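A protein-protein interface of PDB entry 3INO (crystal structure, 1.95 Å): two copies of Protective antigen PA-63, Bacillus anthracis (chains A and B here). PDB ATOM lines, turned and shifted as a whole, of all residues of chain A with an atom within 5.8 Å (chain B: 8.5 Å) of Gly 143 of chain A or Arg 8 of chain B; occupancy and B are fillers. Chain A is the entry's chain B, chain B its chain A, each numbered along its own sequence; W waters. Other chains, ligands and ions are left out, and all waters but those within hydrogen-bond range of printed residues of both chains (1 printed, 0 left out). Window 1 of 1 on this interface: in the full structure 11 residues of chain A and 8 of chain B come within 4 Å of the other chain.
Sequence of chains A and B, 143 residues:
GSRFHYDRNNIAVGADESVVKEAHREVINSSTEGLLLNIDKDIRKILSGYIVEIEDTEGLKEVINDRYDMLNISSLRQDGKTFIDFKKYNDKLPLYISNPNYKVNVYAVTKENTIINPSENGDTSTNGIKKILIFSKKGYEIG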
ATOM      1  N   SER A  30       4.347 -14.540  24.567  1.00  0.00           N
ATOM      2  CA  SER A  30       3.818 -13.287  25.039  1.00  0.00           C
ATOM      3  C   SER A  30       2.485 -13.481  25.771  1.00  0.00           C
ATOM      4  O   SER A  30       1.696 -14.362  25.454  1.00  0.00           O
ATOM      5  CB  SER A  30       3.698 -12.259  23.908  1.00  0.00           C
ATOM      6  OG  SER A  30       2.698 -12.663  22.975  1.00  0.00           O
ATOM      7  N   SER A  31       2.290 -12.678  26.810  1.00  0.00           N
ATOM      8  CA  SER A  31       1.046 -12.639  27.538  1.00  0.00           C
ATOM      9  C   SER A  31       0.954 -11.285  28.215  1.00  0.00           C
ATOM     10  O   SER A  31       1.850 -10.453  28.106  1.00  0.00           O
ATOM     11  CB  SER A  31       0.967 -13.755  28.576  1.00  0.00           C
ATOM     12  OG  SER A  31       1.781 -13.438  29.704  1.00  0.00           O
ATOM     13  N   THR A  32      -0.137 -11.062  28.925  1.00  0.00           N
ATOM     14  CA  THR A  32      -0.285  -9.853  29.656  1.00  0.00           C
ATOM     15  C   THR A  32       0.619  -9.863  30.886  1.00  0.00           C
ATOM     16  O   THR A  32       0.622  -8.902  31.593  1.00  0.00           O
ATOM     17  CB  THR A  32      -1.696  -9.662  30.069  1.00  0.00           C
ATOM     18  OG1 THR A  32      -2.116 -10.809  30.786  1.00  0.00           O
ATOM     19  CG2 THR A  32      -2.585  -9.461  28.844  1.00  0.00           C
ATOM     20  N   ILE A  97      -5.932  -5.340  29.452  1.00  0.00           N
ATOM     21  CA  ILE A  97      -6.114  -4.888  28.080  1.00  0.00           C
ATOM     22  C   ILE A  97      -7.614  -4.810  27.819  1.00  0.00           C
ATOM     23  O   ILE A  97      -8.285  -5.818  27.694  1.00  0.00           O
ATOM     24  CB  ILE A  97      -5.433  -5.817  27.043  1.00  0.00           C
ATOM     25  CG1 ILE A  97      -3.940  -5.906  27.377  1.00  0.00           C
ATOM     26  CG2 ILE A  97      -5.619  -5.272  25.654  1.00  0.00           C
ATOM     27  CD1 ILE A  97      -3.152  -7.082  26.697  1.00  0.00           C
ATOM     28  N   PRO A 100      -9.418  -5.786  22.576  1.00  0.00           N
ATOM     29  CA  PRO A 100      -8.397  -6.598  21.908  1.00  0.00           C
ATOM     30  C   PRO A 100      -7.705  -5.861  20.822  1.00  0.00           C
ATOM     31  O   PRO A 100      -6.741  -6.371  20.246  1.00  0.00           O
ATOM     32  CB  PRO A 100      -9.180  -7.785  21.309  1.00  0.00           C
ATOM     33  CG  PRO A 100     -10.607  -7.350  21.372  1.00  0.00           C
ATOM     34  CD  PRO A 100     -10.731  -6.438  22.529  1.00  0.00           C
ATOM     35  N   LYS A 138      -1.255  -6.284  19.040  1.00  0.00           N
ATOM     36  CA  LYS A 138      -2.565  -6.057  19.574  1.00  0.00           C
ATOM     37  C   LYS A 138      -2.962  -7.131  20.614  1.00  0.00           C
ATOM     38  O   LYS A 138      -2.476  -8.279  20.583  1.00  0.00           O
ATOM     39  CB  LYS A 138      -3.551  -5.958  18.405  1.00  0.00           C
ATOM     40  CG  LYS A 138      -3.394  -4.600  17.715  1.00  0.00           C
ATOM     41  CD  LYS A 138      -3.950  -4.592  16.296  1.00  0.00           C
ATOM     42  CE  LYS A 138      -4.271  -3.181  15.810  1.00  0.00           C
ATOM     43  NZ  LYS A 138      -5.101  -2.394  16.778  1.00  0.00           N
ATOM     44  N   GLY A 139      -3.848  -6.744  21.512  1.00  0.00           N
ATOM     45  CA  GLY A 139      -4.406  -7.653  22.518  1.00  0.00           C
ATOM     46  C   GLY A 139      -4.838  -9.001  21.963  1.00  0.00           C
ATOM     47  O   GLY A 139      -4.562 -10.030  22.556  1.00  0.00           O
ATOM     48  N   TYR A 140      -5.549  -9.012  20.842  1.00  0.00           N
ATOM     49  CA  TYR A 140      -5.945 -10.272  20.266  1.00  0.00           C
ATOM     50  C   TYR A 140      -4.799 -11.184  19.798  1.00  0.00           C
ATOM     51  O   TYR A 140      -5.030 -12.345  19.496  1.00  0.00           O
ATOM     52  CB  TYR A 140      -6.964 -10.035  19.152  1.00  0.00           C
ATOM     53  CG  TYR A 140      -6.426  -9.556  17.853  1.00  0.00           C
ATOM     54  CD1 TYR A 140      -5.914 -10.430  16.914  1.00  0.00           C
ATOM     55  CD2 TYR A 140      -6.508  -8.213  17.532  1.00  0.00           C
ATOM     56  CE1 TYR A 140      -5.419  -9.959  15.683  1.00  0.00           C
ATOM     57  CE2 TYR A 140      -6.016  -7.738  16.342  1.00  0.00           C
ATOM     58  CZ  TYR A 140      -5.470  -8.608  15.441  1.00  0.00           C
ATOM     59  OH  TYR A 140      -5.051  -8.042  14.273  1.00  0.00           O
ATOM     60  N   GLU A 141      -3.576 -10.660  19.728  1.00  0.00           N
ATOM     61  CA  GLU A 141      -2.426 -11.383  19.227  1.00  0.00           C
ATOM     62  C   GLU A 141      -1.494 -11.821  20.345  1.00  0.00           C
ATOM     63  O   GLU A 141      -0.466 -12.367  20.047  1.00  0.00           O
ATOM     64  CB  GLU A 141      -1.571 -10.516  18.312  1.00  0.00           C
ATOM     65  CG  GLU A 141      -2.199 -10.021  17.018  1.00  0.00           C
ATOM     66  CD  GLU A 141      -1.294  -9.051  16.275  1.00  0.00           C
ATOM     67  OE1 GLU A 141      -1.024  -7.915  16.777  1.00  0.00           O
ATOM     68  OE2 GLU A 141      -0.860  -9.406  15.166  1.00  0.00           O
ATOM     69  N   ILE A 142      -1.854 -11.521  21.585  1.00  0.00           N
ATOM     70  CA  ILE A 142      -1.108 -11.831  22.818  1.00  0.00           C
ATOM     71  C   ILE A 142      -1.862 -12.880  23.647  1.00  0.00           C
ATOM     72  O   ILE A 142      -3.055 -12.960  23.557  1.00  0.00           O
ATOM     73  CB  ILE A 142      -0.986 -10.512  23.698  1.00  0.00           C
ATOM     74  CG1 ILE A 142      -0.147  -9.451  22.991  1.00  0.00           C
ATOM     75  CG2 ILE A 142      -0.390 -10.759  25.062  1.00  0.00           C
ATOM     76  CD1 ILE A 142      -0.125  -8.150  23.829  1.00  0.00           C
ATOM     77  N   GLY A 143      -1.190 -13.620  24.535  1.00  0.00           N
ATOM     78  CA  GLY A 143      -1.853 -14.680  25.327  1.00  0.00           C
ATOM     79  C   GLY A 143      -2.569 -14.204  26.562  1.00  0.00           C
ATOM     80  O   GLY A 143      -2.242 -13.175  27.129  1.00  0.00           O
ATOM     81  N   HIS B   5     -14.629 -21.961  30.015  1.00  0.00           N
ATOM     82  CA  HIS B   5     -14.380 -20.571  30.506  1.00  0.00           C
ATOM     83  C   HIS B   5     -13.522 -19.888  29.437  1.00  0.00           C
ATOM     84  O   HIS B   5     -12.600 -20.510  28.949  1.00  0.00           O
ATOM     85  CB  HIS B   5     -13.570 -20.552  31.810  1.00  0.00           C
ATOM     86  CG  HIS B   5     -14.105 -21.402  32.911  1.00  0.00           C
ATOM     87  ND1 HIS B   5     -13.352 -21.690  34.038  1.00  0.00           N
ATOM     88  CD2 HIS B   5     -15.303 -22.000  33.097  1.00  0.00           C
ATOM     89  CE1 HIS B   5     -14.079 -22.419  34.862  1.00  0.00           C
ATOM     90  NE2 HIS B   5     -15.249 -22.649  34.306  1.00  0.00           N
ATOM     91  N   TYR B   6     -13.783 -18.621  29.129  1.00  0.00           N
ATOM     92  CA  TYR B   6     -13.211 -17.937  27.964  1.00  0.00           C
ATOM     93  C   TYR B   6     -12.379 -16.748  28.441  1.00  0.00           C
ATOM     94  O   TYR B   6     -12.707 -16.174  29.417  1.00  0.00           O
ATOM     95  CB  TYR B   6     -14.319 -17.439  27.013  1.00  0.00           C
ATOM     96  CG  TYR B   6     -14.956 -18.588  26.297  1.00  0.00           C
ATOM     97  CD1 TYR B   6     -14.452 -19.030  25.090  1.00  0.00           C
ATOM     98  CD2 TYR B   6     -16.004 -19.252  26.837  1.00  0.00           C
ATOM     99  CE1 TYR B   6     -14.955 -20.111  24.473  1.00  0.00           C
ATOM    100  CE2 TYR B   6     -16.493 -20.358  26.222  1.00  0.00           C
ATOM    101  CZ  TYR B   6     -15.983 -20.748  25.043  1.00  0.00           C
ATOM    102  OH  TYR B   6     -16.492 -21.835  24.435  1.00  0.00           O
ATOM    103  N   ASP B   7     -11.281 -16.439  27.782  1.00  0.00           N
ATOM    104  CA  ASP B   7     -10.432 -15.279  28.219  1.00  0.00           C
ATOM    105  C   ASP B   7     -10.913 -13.980  27.553  1.00  0.00           C
ATOM    106  O   ASP B   7     -12.006 -13.941  26.990  1.00  0.00           O
ATOM    107  CB  ASP B   7      -8.978 -15.565  27.946  1.00  0.00           C
ATOM    108  CG  ASP B   7      -8.648 -15.601  26.470  1.00  0.00           C
ATOM    109  OD1 ASP B   7      -9.491 -15.213  25.594  1.00  0.00           O
ATOM    110  OD2 ASP B   7      -7.536 -16.034  26.148  1.00  0.00           O
ATOM    111  N   ARG B   8     -10.120 -12.911  27.640  1.00  0.00           N
ATOM    112  CA  ARG B   8     -10.553 -11.594  27.208  1.00  0.00           C
ATOM    113  C   ARG B   8     -10.607 -11.595  25.691  1.00  0.00           C
ATOM    114  O   ARG B   8     -11.264 -10.743  25.098  1.00  0.00           O
ATOM    115  CB  ARG B   8      -9.580 -10.514  27.724  1.00  0.00           C
ATOM    116  CG  ARG B   8      -8.214 -10.677  27.102  1.00  0.00           C
ATOM    117  CD  ARG B   8      -7.061  -9.672  27.558  1.00  0.00           C
ATOM    118  NE  ARG B   8      -6.081  -9.800  26.493  1.00  0.00           N
ATOM    119  CZ  ARG B   8      -5.101 -10.685  26.476  1.00  0.00           C
ATOM    120  NH1 ARG B   8      -4.889 -11.419  27.532  1.00  0.00           N
ATOM    121  NH2 ARG B   8      -4.306 -10.802  25.431  1.00  0.00           N
ATOM    122  N   ASN B   9     -10.001 -12.585  25.036  1.00  0.00           N
ATOM    123  CA  ASN B   9     -10.115 -12.695  23.557  1.00  0.00           C
ATOM    124  C   ASN B   9     -11.182 -13.718  23.100  1.00  0.00           C
ATOM    125  O   ASN B   9     -11.210 -14.097  21.954  1.00  0.00           O
ATOM    126  CB  ASN B   9      -8.773 -13.062  22.890  1.00  0.00           C
ATOM    127  CG  ASN B   9      -7.739 -11.946  22.975  1.00  0.00           C
ATOM    128  OD1 ASN B   9      -8.062 -10.772  22.858  1.00  0.00           O
ATOM    129  ND2 ASN B   9      -6.492 -12.324  23.246  1.00  0.00           N
ATOM    130  N   ASN B  10     -12.034 -14.157  24.013  1.00  0.00           N
ATOM    131  CA  ASN B  10     -13.056 -15.149  23.719  1.00  0.00           C
ATOM    132  C   ASN B  10     -12.413 -16.443  23.227  1.00  0.00           C
ATOM    133  O   ASN B  10     -12.949 -17.160  22.380  1.00  0.00           O
ATOM    134  CB  ASN B  10     -14.104 -14.560  22.754  1.00  0.00           C
ATOM    135  CG  ASN B  10     -14.984 -13.516  23.431  1.00  0.00           C
ATOM    136  OD1 ASN B  10     -15.305 -13.654  24.599  1.00  0.00           O
ATOM    137  ND2 ASN B  10     -15.375 -12.474  22.709  1.00  0.00           N
ATOM    138  N   ILE B  11     -11.234 -16.744  23.776  1.00  0.00           N
ATOM    139  CA  ILE B  11     -10.555 -18.039  23.567  1.00  0.00           C
ATOM    140  C   ILE B  11     -10.757 -18.906  24.833  1.00  0.00           C
ATOM    141  O   ILE B  11     -10.589 -18.416  25.963  1.00  0.00           O
ATOM    142  CB  ILE B  11      -9.035 -17.849  23.266  1.00  0.00           C
ATOM    143  CG1 ILE B  11      -8.779 -17.024  21.985  1.00  0.00           C
ATOM    144  CG2 ILE B  11      -8.348 -19.127  23.026  1.00  0.00           C
ATOM    145  CD1 ILE B  11      -9.522 -17.472  20.744  1.00  0.00           C
ATOM    146  N   ALA B  12     -11.159 -20.161  24.648  1.00  0.00           N
ATOM    147  CA  ALA B  12     -11.336 -21.104  25.769  1.00  0.00           C
ATOM    148  C   ALA B  12      -9.980 -21.374  26.477  1.00  0.00           C
ATOM    149  O   ALA B  12      -9.006 -21.768  25.824  1.00  0.00           O
ATOM    150  CB  ALA B  12     -11.943 -22.463  25.263  1.00  0.00           C
ATOM    151  N   VAL B  13      -9.956 -21.241  27.805  1.00  0.00           N
ATOM    152  CA  VAL B  13      -8.753 -21.328  28.573  1.00  0.00           C
ATOM    153  C   VAL B  13      -8.973 -22.162  29.879  1.00  0.00           C
ATOM    154  O   VAL B  13      -8.062 -22.281  30.690  1.00  0.00           O
ATOM    155  CB  VAL B  13      -8.213 -19.918  28.994  1.00  0.00           C
ATOM    156  CG1 VAL B  13      -7.644 -19.203  27.832  1.00  0.00           C
ATOM    157  CG2 VAL B  13      -9.348 -19.059  29.721  1.00  0.00           C
ATOM    158  N   ILE B 116       2.853 -19.127  34.381  1.00  0.00           N
ATOM    159  CA  ILE B 116       3.555 -18.734  33.173  1.00  0.00           C
ATOM    160  C   ILE B 116       5.027 -18.375  33.432  1.00  0.00           C
ATOM    161  O   ILE B 116       5.877 -18.704  32.653  1.00  0.00           O
ATOM    162  CB  ILE B 116       2.848 -17.456  32.595  1.00  0.00           C
ATOM    163  CG1 ILE B 116       1.434 -17.803  32.089  1.00  0.00           C
ATOM    164  CG2 ILE B 116       3.715 -16.763  31.514  1.00  0.00           C
ATOM    165  CD1 ILE B 116       0.605 -16.605  31.775  1.00  0.00           C
HETATM  166  O   HOH W   1      -7.030  -8.581  24.083  1.00  0.00           O
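The backbone carbonyl oxygen (O) of Gly 139 of chain A sits at hydrogen-bond distance from the guanidinium group (NH2) of Arg 8 of chain B (3.0 Å).
The guanidinium group (NH2) of Arg 8 of chain B sits at hydrogen-bond distance from the backbone carbonyl oxygen (O) of Ile 142 of chain A, at 3.1 Å.
The side-chain amide nitrogen (ND2) of Asn 9 of chain B is in hydrogen-bond range of the backbone carbonyl oxygen (O) of Gly 139 of chain A (3.1 Å).
The backbone carbonyl oxygen (O) of Gly 143 of chain A is in hydrogen-bond range of the guanidinium group (NH1) of Arg 8 of chain B (3.2 Å).
The backbone carbonyl oxygen of Gly 143 of chain A is in hydrogen-bond range of the backbone NH of Thr 32 of chain A (3.5 Å).
The backbone NH (N) of Tyr 140 of chain A lies within hydrogen-bond range of the backbone carbonyl oxygen (O) of Pro 100 of chain A (3.0 Å).
The backbone carbonyl oxygen of Ser 30 of chain A lies within hydrogen-bond range of the backbone NH of Gly 143 of chain A (3.1 Å).
OD1 of Asp 7 of chain B sits at hydrogen-bond distance from N of Asn 9 of chain B, 2.7 Å away.
NH2 of Arg 8 of chain B sits close to ND2 of Asn 9 of chain B, 3.4 Å away.
The backbone carbonyl oxygen (O) of Pro 100 of chain A is in hydrogen-bond range of the backbone NH (N) of Gly 139 of chain A (3.2 Å).
Among the printed residues, pairs that only touch across the chains: Ser 31 of chain A with Ile 116 of chain B (3.96 Å), Thr 32 of chain A with Arg 8 of chain B (3.3 Å), Pro 100 of chain A with Asn 9 of chain B (3.5 Å), Tyr 140 of chain A with Asn 9 of chain B (3.4 Å) and Ile 142 of chain A with Asn 9 of chain B (3.5 Å).
Printed residues of chain A within 4 Å of Arg 8 of chain B: Thr 32, Gly 139, Ile 142 and Gly 143.
Printed residues of chain B within 4 Å of Gly 139 of chain A: Arg 8 (3.0 Å) and Asn 9 (3.1 Å).
Of the printed residues of chain B, Tyr 140 of chain A touches Asn 9.
Printed residues of chain A within 4 Å of Ile 116 of chain B: Ser 31 (3.96 Å).
Printed residues of chain B within 4 Å of Ser 31 of chain A: Ile 116.
Tyr 6 of chain B touches none of the printed residues of chain A.
Glu 141 of chain A touches none of the printed residues of chain B.
The nearest printed residue of chain A that does not touch Arg 8 of chain B is Ile 97 of chain A (4.001 Å).
Hydrophobic or aromatic side chains of chain B within 4 Å of the printed part of chain A: Ile 116.
Of the 11 printed residues of chain A, 7 touch a printed residue of chain B.
No position is printed for both chains.
Water W1 lies within hydrogen-bond range of OD1 of Asn 9 of chain B (2.7 Å), NE of Arg 8 of chain B (2.9 Å) and O of Gly 139 of chain A (3.2 Å).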
